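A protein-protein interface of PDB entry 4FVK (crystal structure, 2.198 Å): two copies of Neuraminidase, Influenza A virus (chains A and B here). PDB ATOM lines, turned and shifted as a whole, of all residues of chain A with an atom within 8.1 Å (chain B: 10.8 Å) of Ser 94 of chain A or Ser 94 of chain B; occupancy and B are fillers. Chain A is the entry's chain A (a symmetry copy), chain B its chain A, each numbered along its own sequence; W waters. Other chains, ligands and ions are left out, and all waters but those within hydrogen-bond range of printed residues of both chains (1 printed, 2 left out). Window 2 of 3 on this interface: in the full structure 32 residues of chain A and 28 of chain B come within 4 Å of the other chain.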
ATOM      1  N   ASP A  40      -4.608  19.813  24.805  1.00  0.00           N
ATOM      2  CA  ASP A  40      -3.153  19.629  24.652  1.00  0.00           C
ATOM      3  C   ASP A  40      -2.647  19.813  23.237  1.00  0.00           C
ATOM      4  O   ASP A  40      -1.564  19.347  22.889  1.00  0.00           O
ATOM      5  CB  ASP A  40      -2.687  18.262  25.175  1.00  0.00           C
ATOM      6  CG  ASP A  40      -2.649  18.204  26.680  1.00  0.00           C
ATOM      7  OD1 ASP A  40      -2.984  17.139  27.243  1.00  0.00           O
ATOM      8  OD2 ASP A  40      -2.290  19.230  27.293  1.00  0.00           O
ATOM      9  N   LEU A  41      -3.431  20.483  22.407  1.00  0.00           N
ATOM     10  CA  LEU A  41      -2.991  20.732  21.058  1.00  0.00           C
ATOM     11  C   LEU A  41      -2.292  22.085  21.014  1.00  0.00           C
ATOM     12  O   LEU A  41      -2.815  23.058  21.514  1.00  0.00           O
ATOM     13  CB  LEU A  41      -4.193  20.717  20.113  1.00  0.00           C
ATOM     14  CG  LEU A  41      -3.872  20.314  18.685  1.00  0.00           C
ATOM     15  CD1 LEU A  41      -3.505  18.836  18.688  1.00  0.00           C
ATOM     16  CD2 LEU A  41      -5.066  20.595  17.773  1.00  0.00           C
ATOM     17  N   ILE A  42      -1.109  22.140  20.427  1.00  0.00           N
ATOM     18  CA  ILE A  42      -0.475  23.421  20.132  1.00  0.00           C
ATOM     19  C   ILE A  42      -1.117  24.018  18.866  1.00  0.00           C
ATOM     20  O   ILE A  42      -1.124  23.380  17.810  1.00  0.00           O
ATOM     21  CB  ILE A  42       1.018  23.218  19.873  1.00  0.00           C
ATOM     22  CG1 ILE A  42       1.643  22.354  20.977  1.00  0.00           C
ATOM     23  CG2 ILE A  42       1.705  24.537  19.730  1.00  0.00           C
ATOM     24  CD1 ILE A  42       3.073  21.949  20.677  1.00  0.00           C
ATOM     25  N   LEU A  65      -2.222  26.849  23.388  1.00  0.00           N
ATOM     26  CA  LEU A  65      -2.405  25.464  23.742  1.00  0.00           C
ATOM     27  C   LEU A  65      -3.846  25.317  24.184  1.00  0.00           C
ATOM     28  O   LEU A  65      -4.314  26.079  25.017  1.00  0.00           O
ATOM     29  CB  LEU A  65      -1.443  25.067  24.870  1.00  0.00           C
ATOM     30  CG  LEU A  65      -1.374  23.573  25.203  1.00  0.00           C
ATOM     31  CD1 LEU A  65      -0.818  22.742  24.044  1.00  0.00           C
ATOM     32  CD2 LEU A  65      -0.553  23.353  26.486  1.00  0.00           C
ATOM     33  N   THR A  85       6.915  19.121  14.105  1.00  0.00           N
ATOM     34  CA  THR A  85       6.067  17.939  14.323  1.00  0.00           C
ATOM     35  C   THR A  85       6.105  17.089  13.044  1.00  0.00           C
ATOM     36  O   THR A  85       6.083  17.645  11.959  1.00  0.00           O
ATOM     37  CB  THR A  85       4.588  18.366  14.555  1.00  0.00           C
ATOM     38  OG1 THR A  85       4.522  19.282  15.652  1.00  0.00           O
ATOM     39  CG2 THR A  85       3.653  17.174  14.825  1.00  0.00           C
ATOM     40  N   PRO A  86       6.140  15.743  13.162  1.00  0.00           N
ATOM     41  CA  PRO A  86       6.071  14.901  11.951  1.00  0.00           C
ATOM     42  C   PRO A  86       4.753  15.124  11.181  1.00  0.00           C
ATOM     43  O   PRO A  86       3.748  15.404  11.838  1.00  0.00           O
ATOM     44  CB  PRO A  86       6.147  13.474  12.501  1.00  0.00           C
ATOM     45  CG  PRO A  86       6.788  13.618  13.856  1.00  0.00           C
ATOM     46  CD  PRO A  86       6.374  14.959  14.386  1.00  0.00           C
ATOM     47  N   SER A  89       1.517  13.334  12.389  1.00  0.00           N
ATOM     48  CA  SER A  89       1.017  13.441  13.761  1.00  0.00           C
ATOM     49  C   SER A  89       0.316  14.742  14.036  1.00  0.00           C
ATOM     50  O   SER A  89       0.697  15.791  13.510  1.00  0.00           O
ATOM     51  CB  SER A  89       2.156  13.345  14.790  1.00  0.00           C
ATOM     52  OG  SER A  89       3.024  12.261  14.530  1.00  0.00           O
ATOM     53  N   ALA A  90      -0.654  14.692  14.938  1.00  0.00           N
ATOM     54  CA  ALA A  90      -1.297  15.901  15.418  1.00  0.00           C
ATOM     55  C   ALA A  90      -0.268  16.684  16.193  1.00  0.00           C
ATOM     56  O   ALA A  90       0.681  16.097  16.681  1.00  0.00           O
ATOM     57  CB  ALA A  90      -2.452  15.549  16.312  1.00  0.00           C
ATOM     58  N   SER A  91      -0.451  17.988  16.338  1.00  0.00           N
ATOM     59  CA  SER A  91       0.570  18.805  16.972  1.00  0.00           C
ATOM     60  C   SER A  91       0.366  18.945  18.500  1.00  0.00           C
ATOM     61  O   SER A  91       0.048  20.016  18.984  1.00  0.00           O
ATOM     62  CB  SER A  91       0.672  20.182  16.271  1.00  0.00           C
ATOM     63  OG  SER A  91      -0.566  20.867  16.331  1.00  0.00           O
ATOM     64  N   THR A  92       0.552  17.853  19.244  1.00  0.00           N
ATOM     65  CA  THR A  92       0.427  17.877  20.709  1.00  0.00           C
ATOM     66  C   THR A  92       1.754  18.136  21.379  1.00  0.00           C
ATOM     67  O   THR A  92       2.804  18.051  20.742  1.00  0.00           O
ATOM     68  CB  THR A  92      -0.068  16.523  21.254  1.00  0.00           C
ATOM     69  OG1 THR A  92       0.865  15.507  20.878  1.00  0.00           O
ATOM     70  CG2 THR A  92      -1.413  16.184  20.668  1.00  0.00           C
ATOM     71  N   LEU A  93       1.699  18.427  22.678  1.00  0.00           N
ATOM     72  CA  LEU A  93       2.891  18.628  23.494  1.00  0.00           C
ATOM     73  C   LEU A  93       3.801  17.406  23.502  1.00  0.00           C
ATOM     74  O   LEU A  93       5.016  17.531  23.509  1.00  0.00           O
ATOM     75  CB  LEU A  93       2.498  18.944  24.941  1.00  0.00           C
ATOM     76  CG  LEU A  93       2.286  20.403  25.322  1.00  0.00           C
ATOM     77  CD1 LEU A  93       2.051  20.507  26.815  1.00  0.00           C
ATOM     78  CD2 LEU A  93       3.486  21.264  24.907  1.00  0.00           C
ATOM     79  N   SER A  94       3.223  16.213  23.502  1.00  0.00           N
ATOM     80  CA  SER A  94       4.060  15.018  23.608  1.00  0.00           C
ATOM     81  C   SER A  94       4.779  14.731  22.297  1.00  0.00           C
ATOM     82  O   SER A  94       5.787  14.031  22.254  1.00  0.00           O
ATOM     83  CB  SER A  94       3.240  13.787  24.058  1.00  0.00           C
ATOM     84  OG  SER A  94       2.067  13.624  23.271  1.00  0.00           O
ATOM     85  N   THR A  95       4.260  15.278  21.218  1.00  0.00           N
ATOM     86  CA  THR A  95       4.755  14.891  19.916  1.00  0.00           C
ATOM     87  C   THR A  95       5.485  16.027  19.163  1.00  0.00           C
ATOM     88  O   THR A  95       6.095  15.787  18.121  1.00  0.00           O
ATOM     89  CB  THR A  95       3.586  14.371  19.069  1.00  0.00           C
ATOM     90  OG1 THR A  95       4.075  13.492  18.058  1.00  0.00           O
ATOM     91  CG2 THR A  95       2.882  15.524  18.427  1.00  0.00           C
ATOM     92  N   SER A  96       5.418  17.254  19.671  1.00  0.00           N
ATOM     93  CA  SER A  96       6.037  18.392  18.978  1.00  0.00           C
ATOM     94  C   SER A  96       7.291  18.821  19.717  1.00  0.00           C
ATOM     95  O   SER A  96       7.369  18.689  20.934  1.00  0.00           O
ATOM     96  CB  SER A  96       5.074  19.570  18.918  1.00  0.00           C
ATOM     97  OG  SER A  96       3.814  19.152  18.458  1.00  0.00           O
ATOM     98  N   GLU A  97       8.270  19.339  18.989  1.00  0.00           N
ATOM     99  CA  GLU A  97       9.533  19.709  19.605  1.00  0.00           C
ATOM    100  C   GLU A  97       9.810  21.213  19.471  1.00  0.00           C
ATOM    101  O   GLU A  97       9.745  21.746  18.383  1.00  0.00           O
ATOM    102  CB  GLU A  97      10.675  18.908  18.963  1.00  0.00           C
ATOM    103  CG  GLU A  97      12.047  19.307  19.468  1.00  0.00           C
ATOM    104  CD  GLU A  97      13.156  18.931  18.507  1.00  0.00           C
ATOM    105  OE1 GLU A  97      12.857  18.312  17.462  1.00  0.00           O
ATOM    106  OE2 GLU A  97      14.330  19.264  18.797  1.00  0.00           O
ATOM    107  N   PHE B  31       9.181  27.085  28.545  1.00  0.00           N
ATOM    108  CA  PHE B  31       7.788  26.867  28.180  1.00  0.00           C
ATOM    109  C   PHE B  31       6.972  27.947  28.892  1.00  0.00           C
ATOM    110  O   PHE B  31       7.141  28.174  30.094  1.00  0.00           O
ATOM    111  CB  PHE B  31       7.339  25.431  28.502  1.00  0.00           C
ATOM    112  CG  PHE B  31       7.721  24.442  27.431  1.00  0.00           C
ATOM    113  CD1 PHE B  31       8.970  23.846  27.436  1.00  0.00           C
ATOM    114  CD2 PHE B  31       6.855  24.176  26.372  1.00  0.00           C
ATOM    115  CE1 PHE B  31       9.339  22.964  26.421  1.00  0.00           C
ATOM    116  CE2 PHE B  31       7.206  23.283  25.348  1.00  0.00           C
ATOM    117  CZ  PHE B  31       8.445  22.677  25.369  1.00  0.00           C
ATOM    118  N   TRP B  33       4.400  28.870  30.514  1.00  0.00           N
ATOM    119  CA  TRP B  33       3.243  28.626  31.381  1.00  0.00           C
ATOM    120  C   TRP B  33       2.937  29.821  32.284  1.00  0.00           C
ATOM    121  O   TRP B  33       3.796  30.661  32.520  1.00  0.00           O
ATOM    122  CB  TRP B  33       3.439  27.377  32.240  1.00  0.00           C
ATOM    123  CG  TRP B  33       3.959  26.156  31.494  1.00  0.00           C
ATOM    124  CD1 TRP B  33       4.965  25.318  31.903  1.00  0.00           C
ATOM    125  CD2 TRP B  33       3.511  25.652  30.224  1.00  0.00           C
ATOM    126  NE1 TRP B  33       5.164  24.334  30.977  1.00  0.00           N
ATOM    127  CE2 TRP B  33       4.289  24.508  29.936  1.00  0.00           C
ATOM    128  CE3 TRP B  33       2.534  26.064  29.294  1.00  0.00           C
ATOM    129  CZ2 TRP B  33       4.128  23.766  28.775  1.00  0.00           C
ATOM    130  CZ3 TRP B  33       2.361  25.319  28.132  1.00  0.00           C
ATOM    131  CH2 TRP B  33       3.159  24.182  27.876  1.00  0.00           C
ATOM    132  N   PRO B  38      -0.858  23.168  31.320  1.00  0.00           N
ATOM    133  CA  PRO B  38      -1.607  21.955  30.967  1.00  0.00           C
ATOM    134  C   PRO B  38      -1.526  20.909  32.064  1.00  0.00           C
ATOM    135  O   PRO B  38      -0.598  20.963  32.887  1.00  0.00           O
ATOM    136  CB  PRO B  38      -0.871  21.437  29.733  1.00  0.00           C
ATOM    137  CG  PRO B  38       0.543  21.971  29.881  1.00  0.00           C
ATOM    138  CD  PRO B  38       0.369  23.328  30.515  1.00  0.00           C
ATOM    139  N   GLY B  39      -2.475  19.971  32.082  1.00  0.00           N
ATOM    140  CA  GLY B  39      -2.443  18.879  33.045  1.00  0.00           C
ATOM    141  C   GLY B  39      -1.353  17.877  32.686  1.00  0.00           C
ATOM    142  O   GLY B  39      -0.853  17.892  31.560  1.00  0.00           O
ATOM    143  N   ASP B  40      -0.986  17.013  33.633  1.00  0.00           N
ATOM    144  CA  ASP B  40       0.058  15.992  33.430  1.00  0.00           C
ATOM    145  C   ASP B  40       1.462  16.549  33.326  1.00  0.00           C
ATOM    146  O   ASP B  40       2.362  15.894  32.805  1.00  0.00           O
ATOM    147  CB  ASP B  40      -0.225  15.117  32.200  1.00  0.00           C
ATOM    148  CG  ASP B  40      -1.318  14.109  32.449  1.00  0.00           C
ATOM    149  OD1 ASP B  40      -2.112  13.851  31.519  1.00  0.00           O
ATOM    150  OD2 ASP B  40      -1.380  13.586  33.581  1.00  0.00           O
ATOM    151  N   LEU B  41       1.657  17.766  33.808  1.00  0.00           N
ATOM    152  CA  LEU B  41       2.979  18.339  33.781  1.00  0.00           C
ATOM    153  C   LEU B  41       3.674  18.028  35.100  1.00  0.00           C
ATOM    154  O   LEU B  41       3.106  18.233  36.151  1.00  0.00           O
ATOM    155  CB  LEU B  41       2.881  19.850  33.567  1.00  0.00           C
ATOM    156  CG  LEU B  41       4.085  20.472  32.885  1.00  0.00           C
ATOM    157  CD1 LEU B  41       4.104  19.991  31.440  1.00  0.00           C
ATOM    158  CD2 LEU B  41       4.012  21.997  32.968  1.00  0.00           C
ATOM    159  N   ILE B  42       4.895  17.524  35.041  1.00  0.00           N
ATOM    160  CA  ILE B  42       5.721  17.413  36.239  1.00  0.00           C
ATOM    161  C   ILE B  42       6.321  18.794  36.563  1.00  0.00           C
ATOM    162  O   ILE B  42       6.999  19.392  35.723  1.00  0.00           O
ATOM    163  CB  ILE B  42       6.866  16.429  35.996  1.00  0.00           C
ATOM    164  CG1 ILE B  42       6.335  15.129  35.377  1.00  0.00           C
ATOM    165  CG2 ILE B  42       7.621  16.187  37.262  1.00  0.00           C
ATOM    166  CD1 ILE B  42       7.438  14.191  34.926  1.00  0.00           C
ATOM    167  N   PHE B  60      16.173  17.409  36.592  1.00  0.00           N
ATOM    168  CA  PHE B  60      15.428  18.119  37.626  1.00  0.00           C
ATOM    169  C   PHE B  60      14.857  17.219  38.706  1.00  0.00           C
ATOM    170  O   PHE B  60      14.664  16.032  38.485  1.00  0.00           O
ATOM    171  CB  PHE B  60      14.287  18.935  37.004  1.00  0.00           C
ATOM    172  CG  PHE B  60      13.249  18.098  36.261  1.00  0.00           C
ATOM    173  CD1 PHE B  60      13.448  17.725  34.947  1.00  0.00           C
ATOM    174  CD2 PHE B  60      12.068  17.719  36.874  1.00  0.00           C
ATOM    175  CE1 PHE B  60      12.489  16.992  34.263  1.00  0.00           C
ATOM    176  CE2 PHE B  60      11.090  16.999  36.188  1.00  0.00           C
ATOM    177  CZ  PHE B  60      11.305  16.630  34.882  1.00  0.00           C
ATOM    178  N   LEU B  65       2.683  17.101  40.248  1.00  0.00           N
ATOM    179  CA  LEU B  65       2.094  16.819  38.962  1.00  0.00           C
ATOM    180  C   LEU B  65       0.796  17.599  38.901  1.00  0.00           C
ATOM    181  O   LEU B  65      -0.012  17.519  39.814  1.00  0.00           O
ATOM    182  CB  LEU B  65       1.836  15.315  38.808  1.00  0.00           C
ATOM    183  CG  LEU B  65       1.414  14.842  37.413  1.00  0.00           C
ATOM    184  CD1 LEU B  65       2.510  15.056  36.367  1.00  0.00           C
ATOM    185  CD2 LEU B  65       0.976  13.368  37.462  1.00  0.00           C
ATOM    186  N   TYR B  83      14.593  13.496  37.533  1.00  0.00           N
ATOM    187  CA  TYR B  83      14.065  13.139  36.226  1.00  0.00           C
ATOM    188  C   TYR B  83      14.879  13.801  35.125  1.00  0.00           C
ATOM    189  O   TYR B  83      15.660  14.709  35.376  1.00  0.00           O
ATOM    190  CB  TYR B  83      12.631  13.630  36.101  1.00  0.00           C
ATOM    191  CG  TYR B  83      11.590  12.866  36.883  1.00  0.00           C
ATOM    192  CD1 TYR B  83      10.708  12.018  36.233  1.00  0.00           C
ATOM    193  CD2 TYR B  83      11.458  13.021  38.258  1.00  0.00           C
ATOM    194  CE1 TYR B  83       9.742  11.363  36.900  1.00  0.00           C
ATOM    195  CE2 TYR B  83      10.476  12.328  38.959  1.00  0.00           C
ATOM    196  CZ  TYR B  83       9.623  11.503  38.265  1.00  0.00           C
ATOM    197  OH  TYR B  83       8.625  10.807  38.905  1.00  0.00           O
ATOM    198  N   LYS B  84      14.657  13.354  33.897  1.00  0.00           N
ATOM    199  CA  LYS B  84      15.335  13.893  32.718  1.00  0.00           C
ATOM    200  C   LYS B  84      14.297  14.051  31.588  1.00  0.00           C
ATOM    201  O   LYS B  84      13.429  13.193  31.422  1.00  0.00           O
ATOM    202  CB  LYS B  84      16.424  12.905  32.305  1.00  0.00           C
ATOM    203  CG  LYS B  84      17.010  13.064  30.920  1.00  0.00           C
ATOM    204  CD  LYS B  84      18.162  12.067  30.771  1.00  0.00           C
ATOM    205  CE  LYS B  84      18.384  11.648  29.336  1.00  0.00           C
ATOM    206  NZ  LYS B  84      19.704  10.982  29.165  1.00  0.00           N
ATOM    207  N   THR B  85      14.391  15.147  30.843  1.00  0.00           N
ATOM    208  CA  THR B  85      13.495  15.483  29.725  1.00  0.00           C
ATOM    209  C   THR B  85      14.336  16.161  28.633  1.00  0.00           C
ATOM    210  O   THR B  85      15.205  16.953  28.957  1.00  0.00           O
ATOM    211  CB  THR B  85      12.414  16.505  30.183  1.00  0.00           C
ATOM    212  OG1 THR B  85      11.698  15.973  31.302  1.00  0.00           O
ATOM    213  CG2 THR B  85      11.420  16.869  29.066  1.00  0.00           C
ATOM    214  N   PRO B  86      14.072  15.873  27.340  1.00  0.00           N
ATOM    215  CA  PRO B  86      14.792  16.589  26.269  1.00  0.00           C
ATOM    216  C   PRO B  86      14.524  18.108  26.324  1.00  0.00           C
ATOM    217  O   PRO B  86      13.420  18.479  26.726  1.00  0.00           O
ATOM    218  CB  PRO B  86      14.224  15.981  24.983  1.00  0.00           C
ATOM    219  CG  PRO B  86      13.669  14.646  25.403  1.00  0.00           C
ATOM    220  CD  PRO B  86      13.206  14.800  26.821  1.00  0.00           C
ATOM    221  N   GLY B  88      13.872  20.312  24.200  1.00  0.00           N
ATOM    222  CA  GLY B  88      12.789  20.730  23.334  1.00  0.00           C
ATOM    223  C   GLY B  88      11.392  20.247  23.693  1.00  0.00           C
ATOM    224  O   GLY B  88      10.446  20.544  22.952  1.00  0.00           O
ATOM    225  N   SER B  89      11.234  19.517  24.800  1.00  0.00           N
ATOM    226  CA  SER B  89       9.909  19.023  25.181  1.00  0.00           C
ATOM    227  C   SER B  89       9.439  19.552  26.506  1.00  0.00           C
ATOM    228  O   SER B  89      10.234  19.749  27.429  1.00  0.00           O
ATOM    229  CB  SER B  89       9.888  17.490  25.302  1.00  0.00           C
ATOM    230  OG  SER B  89      10.489  16.855  24.192  1.00  0.00           O
ATOM    231  N   ALA B  90       8.128  19.693  26.636  1.00  0.00           N
ATOM    232  CA  ALA B  90       7.531  20.034  27.914  1.00  0.00           C
ATOM    233  C   ALA B  90       7.754  18.868  28.843  1.00  0.00           C
ATOM    234  O   ALA B  90       7.932  17.760  28.373  1.00  0.00           O
ATOM    235  CB  ALA B  90       6.058  20.278  27.744  1.00  0.00           C
ATOM    236  N   SER B  91       7.721  19.092  30.148  1.00  0.00           N
ATOM    237  CA  SER B  91       8.049  18.028  31.082  1.00  0.00           C
ATOM    238  C   SER B  91       6.810  17.216  31.528  1.00  0.00           C
ATOM    239  O   SER B  91       6.403  17.291  32.674  1.00  0.00           O
ATOM    240  CB  SER B  91       8.839  18.593  32.289  1.00  0.00           C
ATOM    241  OG  SER B  91       8.081  19.580  32.966  1.00  0.00           O
ATOM    242  N   THR B  92       6.221  16.446  30.612  1.00  0.00           N
ATOM    243  CA  THR B  92       5.062  15.600  30.932  1.00  0.00           C
ATOM    244  C   THR B  92       5.481  14.205  31.329  1.00  0.00           C
ATOM    245  O   THR B  92       6.630  13.815  31.122  1.00  0.00           O
ATOM    246  CB  THR B  92       4.132  15.434  29.715  1.00  0.00           C
ATOM    247  OG1 THR B  92       4.872  14.834  28.648  1.00  0.00           O
ATOM    248  CG2 THR B  92       3.627  16.776  29.257  1.00  0.00           C
ATOM    249  N   LEU B  93       4.531  13.450  31.878  1.00  0.00           N
ATOM    250  CA  LEU B  93       4.745  12.055  32.247  1.00  0.00           C
ATOM    251  C   LEU B  93       5.156  11.196  31.056  1.00  0.00           C
ATOM    252  O   LEU B  93       5.971  10.296  31.186  1.00  0.00           O
ATOM    253  CB  LEU B  93       3.467  11.461  32.848  1.00  0.00           C
ATOM    254  CG  LEU B  93       3.264  11.576  34.352  1.00  0.00           C
ATOM    255  CD1 LEU B  93       2.024  10.805  34.756  1.00  0.00           C
ATOM    256  CD2 LEU B  93       4.490  11.060  35.117  1.00  0.00           C
ATOM    257  N   SER B  94       4.597  11.467  29.885  1.00  0.00           N
ATOM    258  CA  SER B  94       4.892  10.605  28.740  1.00  0.00           C
ATOM    259  C   SER B  94       6.289  10.869  28.197  1.00  0.00           C
ATOM    260  O   SER B  94       6.882  10.043  27.508  1.00  0.00           O
ATOM    261  CB  SER B  94       3.836  10.762  27.622  1.00  0.00           C
ATOM    262  OG  SER B  94       3.619  12.129  27.297  1.00  0.00           O
ATOM    263  N   THR B  95       6.825  12.031  28.511  1.00  0.00           N
ATOM    264  CA  THR B  95       8.052  12.445  27.870  1.00  0.00           C
ATOM    265  C   THR B  95       9.259  12.537  28.833  1.00  0.00           C
ATOM    266  O   THR B  95      10.393  12.716  28.389  1.00  0.00           O
ATOM    267  CB  THR B  95       7.829  13.798  27.182  1.00  0.00           C
ATOM    268  OG1 THR B  95       8.765  13.960  26.119  1.00  0.00           O
ATOM    269  CG2 THR B  95       8.010  14.899  28.177  1.00  0.00           C
ATOM    270  N   SER B  96       9.023  12.429  30.137  1.00  0.00           N
ATOM    271  CA  SER B  96      10.112  12.567  31.114  1.00  0.00           C
ATOM    272  C   SER B  96      10.458  11.206  31.691  1.00  0.00           C
ATOM    273  O   SER B  96       9.593  10.345  31.809  1.00  0.00           O
ATOM    274  CB  SER B  96       9.698  13.492  32.250  1.00  0.00           C
ATOM    275  OG  SER B  96       9.144  14.679  31.741  1.00  0.00           O
ATOM    276  N   GLU B  97      11.717  11.011  32.055  1.00  0.00           N
ATOM    277  CA  GLU B  97      12.151   9.715  32.550  1.00  0.00           C
ATOM    278  C   GLU B  97      12.657   9.800  33.997  1.00  0.00           C
ATOM    279  O   GLU B  97      13.496  10.623  34.297  1.00  0.00           O
ATOM    280  CB  GLU B  97      13.257   9.159  31.641  1.00  0.00           C
ATOM    281  CG  GLU B  97      13.848   7.857  32.141  1.00  0.00           C
ATOM    282  CD  GLU B  97      15.232   7.590  31.584  1.00  0.00           C
ATOM    283  OE1 GLU B  97      15.712   8.403  30.764  1.00  0.00           O
ATOM    284  OE2 GLU B  97      15.842   6.567  31.975  1.00  0.00           O
ATOM    285  N   MET B  98      12.179   8.929  34.876  1.00  0.00           N
ATOM    286  CA  MET B  98      12.719   8.868  36.235  1.00  0.00           C
ATOM    287  C   MET B  98      14.093   8.177  36.244  1.00  0.00           C
ATOM    288  O   MET B  98      14.236   7.081  35.709  1.00  0.00           O
ATOM    289  CB  MET B  98      11.751   8.136  37.169  1.00  0.00           C
ATOM    290  CG  MET B  98      12.169   8.149  38.624  1.00  0.00           C
ATOM    291  SD  MET B  98      11.258   6.943  39.618  1.00  0.00           S
ATOM    292  CE  MET B  98       9.766   7.847  40.012  1.00  0.00           C
HETATM  293  O   HOH W   1       6.689  19.493  24.085  1.00  0.00           O
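Water W1 lies within hydrogen-bond range of O of Leu 93 of chain A (2.6 Å), N of Ala 90 of chain B (2.9 Å) and O of Ser 96 of chain A (3.3 Å).
Printed residues of chain B within 4 Å of Asp 40 of chain A: Pro 38 (3.6 Å).
No residue of chain B comes within 4 Å of Thr 92 of chain A.
Ser 94 of chain A touches one residue of chain B.
Of the printed residues of chain A, Trp 33 of chain B touches Leu 65 (3.9 Å) and Leu 93 (3.98 Å).
Of the printed residues of chain A, Pro 38 of chain B touches Asp 40, Leu 65 and Leu 93.
Gly 39 of chain B touches none of the printed residues of chain A.
Pro 86 of chain B touches none of the printed residues of chain A.
Of the printed residues of chain A, Gly 88 of chain B touches Glu 97.
Ser 94 of chain B touches just one residue of chain A: Ser 94 (3.7 Å).
The nearest residue of chain B that does not touch Ser 94 of chain A is Thr 95 of chain B (4.9 Å).
The nearest residue of chain A that does not touch Ser 94 of chain B is Leu 93 of chain A (6.5 Å).
The nearest printed residue of chain B that does not touch Leu 65 of chain A is Gly 39 of chain B (6.8 Å).
Among the printed residues, pairs that only touch across the chains: Asp 40 of chain A with Pro 38 of chain B, Leu 65 of chain A with Trp 33 of chain B, Leu 65 of chain A with Pro 38 of chain B, Leu 93 of chain A with Trp 33 of chain B, Leu 93 of chain A with Pro 38 of chain B, Leu 93 of chain A with Ala 90 of chain B, Ser 94 of chain A with Ser 94 of chain B and Glu 97 of chain A with Gly 88 of chain B.
Hydrophobic or aromatic side chains of chain A within 4 Å of the printed part of chain B: Leu 65 and Leu 93.
Of the 24 printed residues of chain B, 5 touch a printed residue of chain A.
Along chain B the printed residues that touch a printed residue of chain A span positions 33 to 94.
Among the printed residues, 8 pairs touch across the chains.
OG1 of Thr 92 of chain B lies within hydrogen-bond range of OG of Ser 94 of chain B, 3.3 Å away.
O of Asp 40 of chain A is in hydrogen-bond range of N of Leu 93 of chain A, at 3.4 Å.
The side-chain hydroxyl (OG1) of Thr 92 of chain A is in hydrogen-bond range of the side-chain hydroxyl (OG) of Ser 94 of chain A, 3.3 Å away.
Leu 93 of chain A touches Ala 90 of chain B, but with the chains exchanged Ala 90 of chain A does not touch Leu 93 of chain B (15.8 Å).
Ser 94 of chain A touches its own counterpart, Ser 94 of chain B.
Positions printed for both chains: 40, 41, 42, 65, 85, 86, 89, 90, 91, 92, 93, 94, 95, 96 and 97.
Of the 8 pairs that touch across the chains among the printed residues, 1 has its exchanged pair printed and touching as well.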
